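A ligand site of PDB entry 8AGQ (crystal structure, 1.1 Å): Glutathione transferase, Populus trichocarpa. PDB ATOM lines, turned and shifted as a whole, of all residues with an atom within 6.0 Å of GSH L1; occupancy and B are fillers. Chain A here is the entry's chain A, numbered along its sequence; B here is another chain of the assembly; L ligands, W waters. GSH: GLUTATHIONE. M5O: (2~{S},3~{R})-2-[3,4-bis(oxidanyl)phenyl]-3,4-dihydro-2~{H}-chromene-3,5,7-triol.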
ATOM      1  N   ALA A  11       2.587  17.324 -10.444  1.00  0.00           N
ATOM      2  CA  ALA A  11       2.040  16.815  -9.190  1.00  0.00           C
ATOM      3  C   ALA A  11       2.709  17.452  -7.978  1.00  0.00           C
ATOM      4  O   ALA A  11       3.901  17.766  -7.956  1.00  0.00           O
ATOM      5  CB  ALA A  11       2.188  15.294  -9.183  1.00  0.00           C
ATOM      6  N   VAL A  12       1.918  17.597  -6.899  1.00  0.00           N
ATOM      7  CA  VAL A  12       2.366  18.286  -5.710  1.00  0.00           C
ATOM      8  C   VAL A  12       3.617  17.693  -5.078  1.00  0.00           C
ATOM      9  O   VAL A  12       4.537  18.427  -4.722  1.00  0.00           O
ATOM     10  CB  VAL A  12       1.189  18.354  -4.704  1.00  0.00           C
ATOM     11  CG1 VAL A  12       1.629  18.623  -3.259  1.00  0.00           C
ATOM     12  CG2 VAL A  12       0.169  19.390  -5.163  1.00  0.00           C
ATOM     13  N   CYS A  13       3.646  16.382  -4.804  1.00  0.00           N
ATOM     14  CA  CYS A  13       4.757  15.867  -3.993  1.00  0.00           C
ATOM     15  C   CYS A  13       6.042  15.802  -4.815  1.00  0.00           C
ATOM     16  O   CYS A  13       7.119  16.125  -4.315  1.00  0.00           O
ATOM     17  CB  CYS A  13       4.456  14.527  -3.323  1.00  0.00           C
ATOM     18  SG  CYS A  13       3.116  14.594  -2.111  1.00  0.00           S
ATOM     19  N   PRO A  14       6.015  15.434  -6.115  1.00  0.00           N
ATOM     20  CA  PRO A  14       7.233  15.610  -6.911  1.00  0.00           C
ATOM     21  C   PRO A  14       7.706  17.065  -6.923  1.00  0.00           C
ATOM     22  O   PRO A  14       8.887  17.320  -6.846  1.00  0.00           O
ATOM     23  CB  PRO A  14       6.841  15.105  -8.283  1.00  0.00           C
ATOM     24  CG  PRO A  14       5.776  14.076  -8.003  1.00  0.00           C
ATOM     25  CD  PRO A  14       4.965  14.721  -6.889  1.00  0.00           C
ATOM     26  N   ARG A  16       7.377  19.284  -4.578  1.00  0.00           N
ATOM     27  CA  ARG A  16       7.987  19.597  -3.306  1.00  0.00           C
ATOM     28  C   ARG A  16       9.474  19.226  -3.344  1.00  0.00           C
ATOM     29  O   ARG A  16      10.341  19.989  -2.901  1.00  0.00           O
ATOM     30  CB  ARG A  16       7.257  18.870  -2.187  1.00  0.00           C
ATOM     31  CG  ARG A  16       7.748  19.141  -0.794  1.00  0.00           C
ATOM     32  CD  ARG A  16       6.877  18.483   0.294  1.00  0.00           C
ATOM     33  NE  ARG A  16       5.480  18.899   0.309  1.00  0.00           N
ATOM     34  CZ  ARG A  16       4.448  18.173  -0.012  1.00  0.00           C
ATOM     35  NH1 ARG A  16       4.557  16.900  -0.291  1.00  0.00           N
ATOM     36  NH2 ARG A  16       3.259  18.736  -0.080  1.00  0.00           N
ATOM     37  N   LEU A  35       0.295   9.126 -13.498  1.00  0.00           N
ATOM     38  CA  LEU A  35      -0.721   8.937 -12.503  1.00  0.00           C
ATOM     39  C   LEU A  35      -2.103   8.854 -13.138  1.00  0.00           C
ATOM     40  O   LEU A  35      -2.932   8.115 -12.676  1.00  0.00           O
ATOM     41  CB  LEU A  35      -0.693  10.084 -11.480  1.00  0.00           C
ATOM     42  CG  LEU A  35       0.630  10.298 -10.765  1.00  0.00           C
ATOM     43  CD1 LEU A  35       0.480  11.377  -9.724  1.00  0.00           C
ATOM     44  CD2 LEU A  35       1.168   9.019 -10.156  1.00  0.00           C
ATOM     45  N   GLN A  40       1.597   4.196 -11.438  1.00  0.00           N
ATOM     46  CA  GLN A  40       2.188   4.082 -10.112  1.00  0.00           C
ATOM     47  C   GLN A  40       1.706   2.861  -9.357  1.00  0.00           C
ATOM     48  O   GLN A  40       2.307   2.538  -8.324  1.00  0.00           O
ATOM     49  CB  GLN A  40       1.905   5.351  -9.301  1.00  0.00           C
ATOM     50  CG  GLN A  40       0.472   5.561  -8.752  1.00  0.00           C
ATOM     51  CD  GLN A  40      -0.587   6.008  -9.714  1.00  0.00           C
ATOM     52  OE1 GLN A  40      -0.426   5.957 -10.935  1.00  0.00           O
ATOM     53  NE2 GLN A  40      -1.728   6.474  -9.195  1.00  0.00           N
ATOM     54  N   LYS A  41       0.627   2.221  -9.829  1.00  0.00           N
ATOM     55  CA  LYS A  41       0.080   1.064  -9.116  1.00  0.00           C
ATOM     56  C   LYS A  41       0.491  -0.253  -9.747  1.00  0.00           C
ATOM     57  O   LYS A  41       0.106  -1.308  -9.214  1.00  0.00           O
ATOM     58  CB  LYS A  41      -1.447   1.111  -9.057  1.00  0.00           C
ATOM     59  CG  LYS A  41      -2.022   2.328  -8.344  1.00  0.00           C
ATOM     60  CD  LYS A  41      -1.480   2.462  -6.936  1.00  0.00           C
ATOM     61  CE  LYS A  41      -2.113   3.569  -6.144  1.00  0.00           C
ATOM     62  NZ  LYS A  41      -1.443   3.802  -4.847  1.00  0.00           N
ATOM     63  N   GLN A  49       8.523   2.386  -5.387  1.00  0.00           N
ATOM     64  CA  GLN A  49       7.775   2.998  -4.303  1.00  0.00           C
ATOM     65  C   GLN A  49       6.669   2.007  -3.947  1.00  0.00           C
ATOM     66  O   GLN A  49       5.725   1.840  -4.690  1.00  0.00           O
ATOM     67  CB  GLN A  49       7.256   4.388  -4.682  1.00  0.00           C
ATOM     68  CG  GLN A  49       7.237   5.384  -3.547  1.00  0.00           C
ATOM     69  CD  GLN A  49       6.140   5.206  -2.520  1.00  0.00           C
ATOM     70  OE1 GLN A  49       5.582   4.126  -2.404  1.00  0.00           O
ATOM     71  NE2 GLN A  49       5.789   6.270  -1.810  1.00  0.00           N
ATOM     72  N   GLY A  52       2.950   2.620  -4.015  1.00  0.00           N
ATOM     73  CA  GLY A  52       2.346   3.072  -5.252  1.00  0.00           C
ATOM     74  C   GLY A  52       2.028   4.541  -5.296  1.00  0.00           C
ATOM     75  O   GLY A  52       0.976   4.941  -5.768  1.00  0.00           O
ATOM     76  N   GLN A  53       2.963   5.353  -4.819  1.00  0.00           N
ATOM     77  CA  GLN A  53       2.839   6.801  -4.833  1.00  0.00           C
ATOM     78  C   GLN A  53       4.132   7.406  -5.331  1.00  0.00           C
ATOM     79  O   GLN A  53       5.184   6.805  -5.264  1.00  0.00           O
ATOM     80  CB  GLN A  53       2.502   7.366  -3.428  1.00  0.00           C
ATOM     81  CG  GLN A  53       1.200   6.825  -2.886  1.00  0.00           C
ATOM     82  CD  GLN A  53       0.816   7.512  -1.618  1.00  0.00           C
ATOM     83  OE1 GLN A  53       1.622   7.733  -0.743  1.00  0.00           O
ATOM     84  NE2 GLN A  53      -0.460   7.839  -1.562  1.00  0.00           N
ATOM     85  N   VAL A  54       4.037   8.654  -5.795  1.00  0.00           N
ATOM     86  CA  VAL A  54       5.211   9.428  -6.205  1.00  0.00           C
ATOM     87  C   VAL A  54       5.421  10.593  -5.229  1.00  0.00           C
ATOM     88  O   VAL A  54       4.451  11.101  -4.669  1.00  0.00           O
ATOM     89  CB  VAL A  54       5.097   9.925  -7.666  1.00  0.00           C
ATOM     90  CG1 VAL A  54       5.007   8.768  -8.627  1.00  0.00           C
ATOM     91  CG2 VAL A  54       3.905  10.865  -7.844  1.00  0.00           C
ATOM     92  N   PRO A  55       6.660  11.065  -5.004  1.00  0.00           N
ATOM     93  CA  PRO A  55       7.866  10.676  -5.719  1.00  0.00           C
ATOM     94  C   PRO A  55       8.684   9.607  -5.034  1.00  0.00           C
ATOM     95  O   PRO A  55       8.540   9.302  -3.854  1.00  0.00           O
ATOM     96  CB  PRO A  55       8.636  12.013  -5.715  1.00  0.00           C
ATOM     97  CG  PRO A  55       8.309  12.575  -4.359  1.00  0.00           C
ATOM     98  CD  PRO A  55       6.842  12.256  -4.179  1.00  0.00           C
ATOM     99  N   PHE A  65      12.076   7.439  -0.641  1.00  0.00           N
ATOM    100  CA  PHE A  65      10.765   7.988  -0.926  1.00  0.00           C
ATOM    101  C   PHE A  65      10.254   8.717   0.321  1.00  0.00           C
ATOM    102  O   PHE A  65      10.971   8.854   1.304  1.00  0.00           O
ATOM    103  CB  PHE A  65       9.821   6.933  -1.512  1.00  0.00           C
ATOM    104  CG  PHE A  65       9.580   5.714  -0.669  1.00  0.00           C
ATOM    105  CD1 PHE A  65      10.374   4.574  -0.766  1.00  0.00           C
ATOM    106  CD2 PHE A  65       8.516   5.695   0.207  1.00  0.00           C
ATOM    107  CE1 PHE A  65      10.080   3.472   0.034  1.00  0.00           C
ATOM    108  CE2 PHE A  65       8.231   4.582   0.970  1.00  0.00           C
ATOM    109  CZ  PHE A  65       9.023   3.474   0.906  1.00  0.00           C
ATOM    110  N   GLU A  66       9.020   9.223   0.214  1.00  0.00           N
ATOM    111  CA  GLU A  66       8.367  10.169   1.148  1.00  0.00           C
ATOM    112  C   GLU A  66       8.975  11.551   0.933  1.00  0.00           C
ATOM    113  O   GLU A  66      10.118  11.830   1.291  1.00  0.00           O
ATOM    114  CB  GLU A  66       8.394   9.739   2.624  1.00  0.00           C
ATOM    115  CG  GLU A  66       7.388   8.617   2.847  1.00  0.00           C
ATOM    116  CD  GLU A  66       5.932   9.062   2.767  1.00  0.00           C
ATOM    117  OE1 GLU A  66       5.649  10.259   3.003  1.00  0.00           O
ATOM    118  OE2 GLU A  66       5.066   8.194   2.469  1.00  0.00           O
ATOM    119  N   SER A  67       8.182  12.425   0.294  1.00  0.00           N
ATOM    120  CA  SER A  67       8.668  13.725  -0.120  1.00  0.00           C
ATOM    121  C   SER A  67       9.348  14.515   1.002  1.00  0.00           C
ATOM    122  O   SER A  67      10.333  15.204   0.739  1.00  0.00           O
ATOM    123  CB  SER A  67       7.520  14.525  -0.728  1.00  0.00           C
ATOM    124  OG  SER A  67       6.494  14.857   0.225  1.00  0.00           O
ATOM    125  N   ARG A  68       8.799  14.470   2.231  1.00  0.00           N
ATOM    126  CA  ARG A  68       9.381  15.287   3.301  1.00  0.00           C
ATOM    127  C   ARG A  68      10.655  14.670   3.839  1.00  0.00           C
ATOM    128  O   ARG A  68      11.494  15.390   4.360  1.00  0.00           O
ATOM    129  CB  ARG A  68       8.346  15.617   4.358  1.00  0.00           C
ATOM    130  CG  ARG A  68       7.175  16.364   3.758  1.00  0.00           C
ATOM    131  CD  ARG A  68       6.017  16.557   4.716  1.00  0.00           C
ATOM    132  NE  ARG A  68       4.825  17.068   4.066  1.00  0.00           N
ATOM    133  CZ  ARG A  68       3.959  16.336   3.372  1.00  0.00           C
ATOM    134  NH1 ARG A  68       4.162  15.033   3.166  1.00  0.00           N
ATOM    135  NH2 ARG A  68       2.880  16.944   2.905  1.00  0.00           N
ATOM    136  N   GLU B 101       7.831   9.168   8.100  1.00  0.00           N
ATOM    137  CA  GLU B 101       6.857   9.693   7.159  1.00  0.00           C
ATOM    138  C   GLU B 101       5.805   8.633   6.814  1.00  0.00           C
ATOM    139  O   GLU B 101       4.622   8.957   6.714  1.00  0.00           O
ATOM    140  CB  GLU B 101       7.599  10.271   5.955  1.00  0.00           C
ATOM    141  CG  GLU B 101       8.453  11.518   6.300  1.00  0.00           C
ATOM    142  CD  GLU B 101       7.649  12.683   6.855  1.00  0.00           C
ATOM    143  OE1 GLU B 101       6.643  13.037   6.237  1.00  0.00           O
ATOM    144  OE2 GLU B 101       8.009  13.249   7.906  1.00  0.00           O
ATOM    145  N   HIS B 105       1.602   9.071   7.864  1.00  0.00           N
ATOM    146  CA  HIS B 105       0.505   9.182   6.917  1.00  0.00           C
ATOM    147  C   HIS B 105      -0.072   7.797   6.600  1.00  0.00           C
ATOM    148  O   HIS B 105      -1.135   7.434   7.078  1.00  0.00           O
ATOM    149  CB  HIS B 105       0.869   9.964   5.666  1.00  0.00           C
ATOM    150  CG  HIS B 105       1.497  11.272   5.951  1.00  0.00           C
ATOM    151  ND1 HIS B 105       0.746  12.412   6.144  1.00  0.00           N
ATOM    152  CD2 HIS B 105       2.792  11.636   6.143  1.00  0.00           C
ATOM    153  CE1 HIS B 105       1.602  13.409   6.384  1.00  0.00           C
ATOM    154  NE2 HIS B 105       2.824  12.971   6.439  1.00  0.00           N
ATOM    155  N   ASN B 106       0.679   6.994   5.832  1.00  0.00           N
ATOM    156  CA  ASN B 106       0.160   5.715   5.384  1.00  0.00           C
ATOM    157  C   ASN B 106      -0.401   4.879   6.529  1.00  0.00           C
ATOM    158  O   ASN B 106      -1.473   4.296   6.394  1.00  0.00           O
ATOM    159  CB  ASN B 106       1.287   4.934   4.689  1.00  0.00           C
ATOM    160  CG  ASN B 106       1.700   5.512   3.364  1.00  0.00           C
ATOM    161  OD1 ASN B 106       0.967   6.321   2.799  1.00  0.00           O
ATOM    162  ND2 ASN B 106       2.851   5.118   2.839  1.00  0.00           N
HETATM  163  N1  GSH L   1       3.280  10.860   1.944  1.00  0.00           N
HETATM  164  CA1 GSH L   1       3.679  10.815   0.502  1.00  0.00           C
HETATM  165  C1  GSH L   1       4.857  11.768   0.237  1.00  0.00           C
HETATM  166  O11 GSH L   1       5.712  11.447  -0.642  1.00  0.00           O
HETATM  167  O12 GSH L   1       4.864  12.840   0.903  1.00  0.00           O
HETATM  168  CB1 GSH L   1       2.473  11.206  -0.342  1.00  0.00           C
HETATM  169  CG1 GSH L   1       2.744  10.901  -1.799  1.00  0.00           C
HETATM  170  CD1 GSH L   1       1.501  11.133  -2.632  1.00  0.00           C
HETATM  171  OE1 GSH L   1       0.388  11.273  -2.127  1.00  0.00           O
HETATM  172  N2  GSH L   1       1.683  11.231  -3.929  1.00  0.00           N
HETATM  173  CA2 GSH L   1       0.647  11.510  -4.863  1.00  0.00           C
HETATM  174  C2  GSH L   1       0.304  10.240  -5.642  1.00  0.00           C
HETATM  175  O2  GSH L   1       1.187   9.450  -5.980  1.00  0.00           O
HETATM  176  CB2 GSH L   1       1.090  12.638  -5.815  1.00  0.00           C
HETATM  177  SG2 GSH L   1       1.191  14.256  -5.004  1.00  0.00           S
HETATM  178  N3  GSH L   1      -0.962  10.118  -5.986  1.00  0.00           N
HETATM  179  CA3 GSH L   1      -1.472   8.979  -6.712  1.00  0.00           C
HETATM  180  C3  GSH L   1      -1.968   7.831  -5.842  1.00  0.00           C
HETATM  181  O31 GSH L   1      -2.313   6.799  -6.450  1.00  0.00           O
HETATM  182  O32 GSH L   1      -1.977   7.999  -4.604  1.00  0.00           O
HETATM  183  OAB M5O L   2      -5.020  10.402  -7.162  1.00  0.00           O
HETATM  184  CAT M5O L   2      -4.255  11.511  -7.407  1.00  0.00           C
HETATM  185  CAK M5O L   2      -3.775  11.720  -8.694  1.00  0.00           C
HETATM  186  CAY M5O L   2      -2.998  12.810  -8.931  1.00  0.00           C
HETATM  187  OAG M5O L   2      -2.559  13.098 -10.184  1.00  0.00           O
HETATM  188  CBD M5O L   2      -2.702  13.742  -7.926  1.00  0.00           C
HETATM  189  CAP M5O L   2      -1.789  14.914  -8.195  1.00  0.00           C
HETATM  190  CAN M5O L   2      -3.965  12.395  -6.381  1.00  0.00           C
HETATM  191  CBC M5O L   2      -3.184  13.498  -6.652  1.00  0.00           C
HETATM  192  OAR M5O L   2      -3.012  14.394  -5.614  1.00  0.00           O
HETATM  193  CBF M5O L   2      -2.646  15.767  -6.012  1.00  0.00           C
HETATM  194  CBE M5O L   2      -1.397  15.650  -6.926  1.00  0.00           C
HETATM  195  OAQ M5O L   2      -0.889  16.933  -7.224  1.00  0.00           O
HETATM  196  CBA M5O L   2      -2.556  16.608  -4.768  1.00  0.00           C
HETATM  197  CAO M5O L   2      -1.740  16.227  -3.732  1.00  0.00           C
HETATM  198  CAV M5O L   2      -1.711  16.966  -2.561  1.00  0.00           C
HETATM  199  OAD M5O L   2      -0.965  16.618  -1.455  1.00  0.00           O
HETATM  200  CAU M5O L   2      -2.428  18.152  -2.478  1.00  0.00           C
HETATM  201  OAC M5O L   2      -2.410  18.933  -1.341  1.00  0.00           O
HETATM  202  CAI M5O L   2      -3.222  18.541  -3.531  1.00  0.00           C
HETATM  203  CAJ M5O L   2      -3.279  17.763  -4.679  1.00  0.00           C
HETATM  204  O   HOH W   1       6.482  13.098   3.426  1.00  0.00           O
HETATM  205  O   HOH W   2      -0.657  13.929  -1.392  1.00  0.00           O
HETATM  206  O   HOH W   3       1.253   8.821   1.802  1.00  0.00           O
HETATM  207  O   HOH W   4      -4.808   5.805  -5.904  1.00  0.00           O
HETATM  208  O   HOH W   5      -2.518   5.837  -3.237  1.00  0.00           O
HETATM  209  O   HOH W   6      -3.215  10.165  -3.236  1.00  0.00           O
HETATM  210  O   HOH W   7      -2.183  12.602  -3.593  1.00  0.00           O
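An oxygen (OAQ) of M5O L2 lies within hydrogen-bond range of the backbone NH of Val 12 (2.9 Å).
The backbone NH (N) of Val 54 lies within hydrogen-bond range of an oxygen (O2) of GSH L1, at 3.0 Å.
N of Ser 67 lies within hydrogen-bond range of O11 of GSH L1, 2.8 Å away.
O12 of GSH L1 sits at hydrogen-bond distance from OG of Ser 67 (2.7 Å).
The side-chain amide nitrogen (NE2) of Gln 53 lies within hydrogen-bond range of an oxygen (O32) of GSH L1, 3.4 Å away.
O31 of GSH L1 is in salt-bridge range of NZ of Lys 41 (3.5 Å).
A nitrogen (N2) of GSH L1 sits at hydrogen-bond distance from the backbone carbonyl oxygen (O) of Val 54, 2.9 Å away.
The side-chain amide nitrogen (NE2) of Gln 40 is in hydrogen-bond range of an oxygen (O31) of GSH L1 (2.8 Å).
OE1 of Glu 66 is in salt-bridge range of N1 of GSH L1 (2.7 Å).
SG of Cys 13 sits close to SG2 of GSH L1, 3.5 Å away.
SG2 of GSH L1 lies close to N of Cys 13, at 3.3 Å.
NH1 of Arg 68 is in salt-bridge range of O12 of GSH L1 (3.2 Å).
The backbone carbonyl oxygen (O) of Gly 52 sits at hydrogen-bond distance from the side-chain amino group (NZ) of Lys 41 (2.8 Å).
The guanidinium group (NH1) of Arg 16 lies within hydrogen-bond range of the side-chain hydroxyl (OG) of Ser 67, 2.9 Å away.
SG of Cys 13 sits at hydrogen-bond distance from NH1 of Arg 16.
OE1 of Gln 49 sits at hydrogen-bond distance from N of Gly 52 (3.4 Å).
Merely in contact with GSH L1: Val 12 (3.9 Å), Gly 52 (3.8 Å) and Pro 55 (3.8 Å).
Hydrophobic or aromatic side chains within 4 Å of GSH L1: Val 54 and Pro 55.
Of the 20 residues printed, 11 come within 4 Å of GSH L1.
Water W5 lies within hydrogen-bond range of O32 of GSH L1 (2.6 Å), NZ of Lys 41 (2.8 Å) and NE2 of Gln 53 (3.3 Å).
Water W3 lies within hydrogen-bond range of OD1 of Asn 106 of chain B (2.7 Å), OE1 of Gln 53 (2.8 Å) and N1 of GSH L1 (2.9 Å).
Water W2 lies within hydrogen-bond range of an oxygen (OAD) of M5O L2 (2.7 Å) and an oxygen (OE1) of GSH L1 (2.9 Å).
Water W1 lies within hydrogen-bond range of OE1 of Glu 101 of chain B, N of Arg 68, OE1 of Glu 66 and O12 of GSH L1.
Water W7 bridges OAR of M5O L2 and OE1 of GSH L1.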
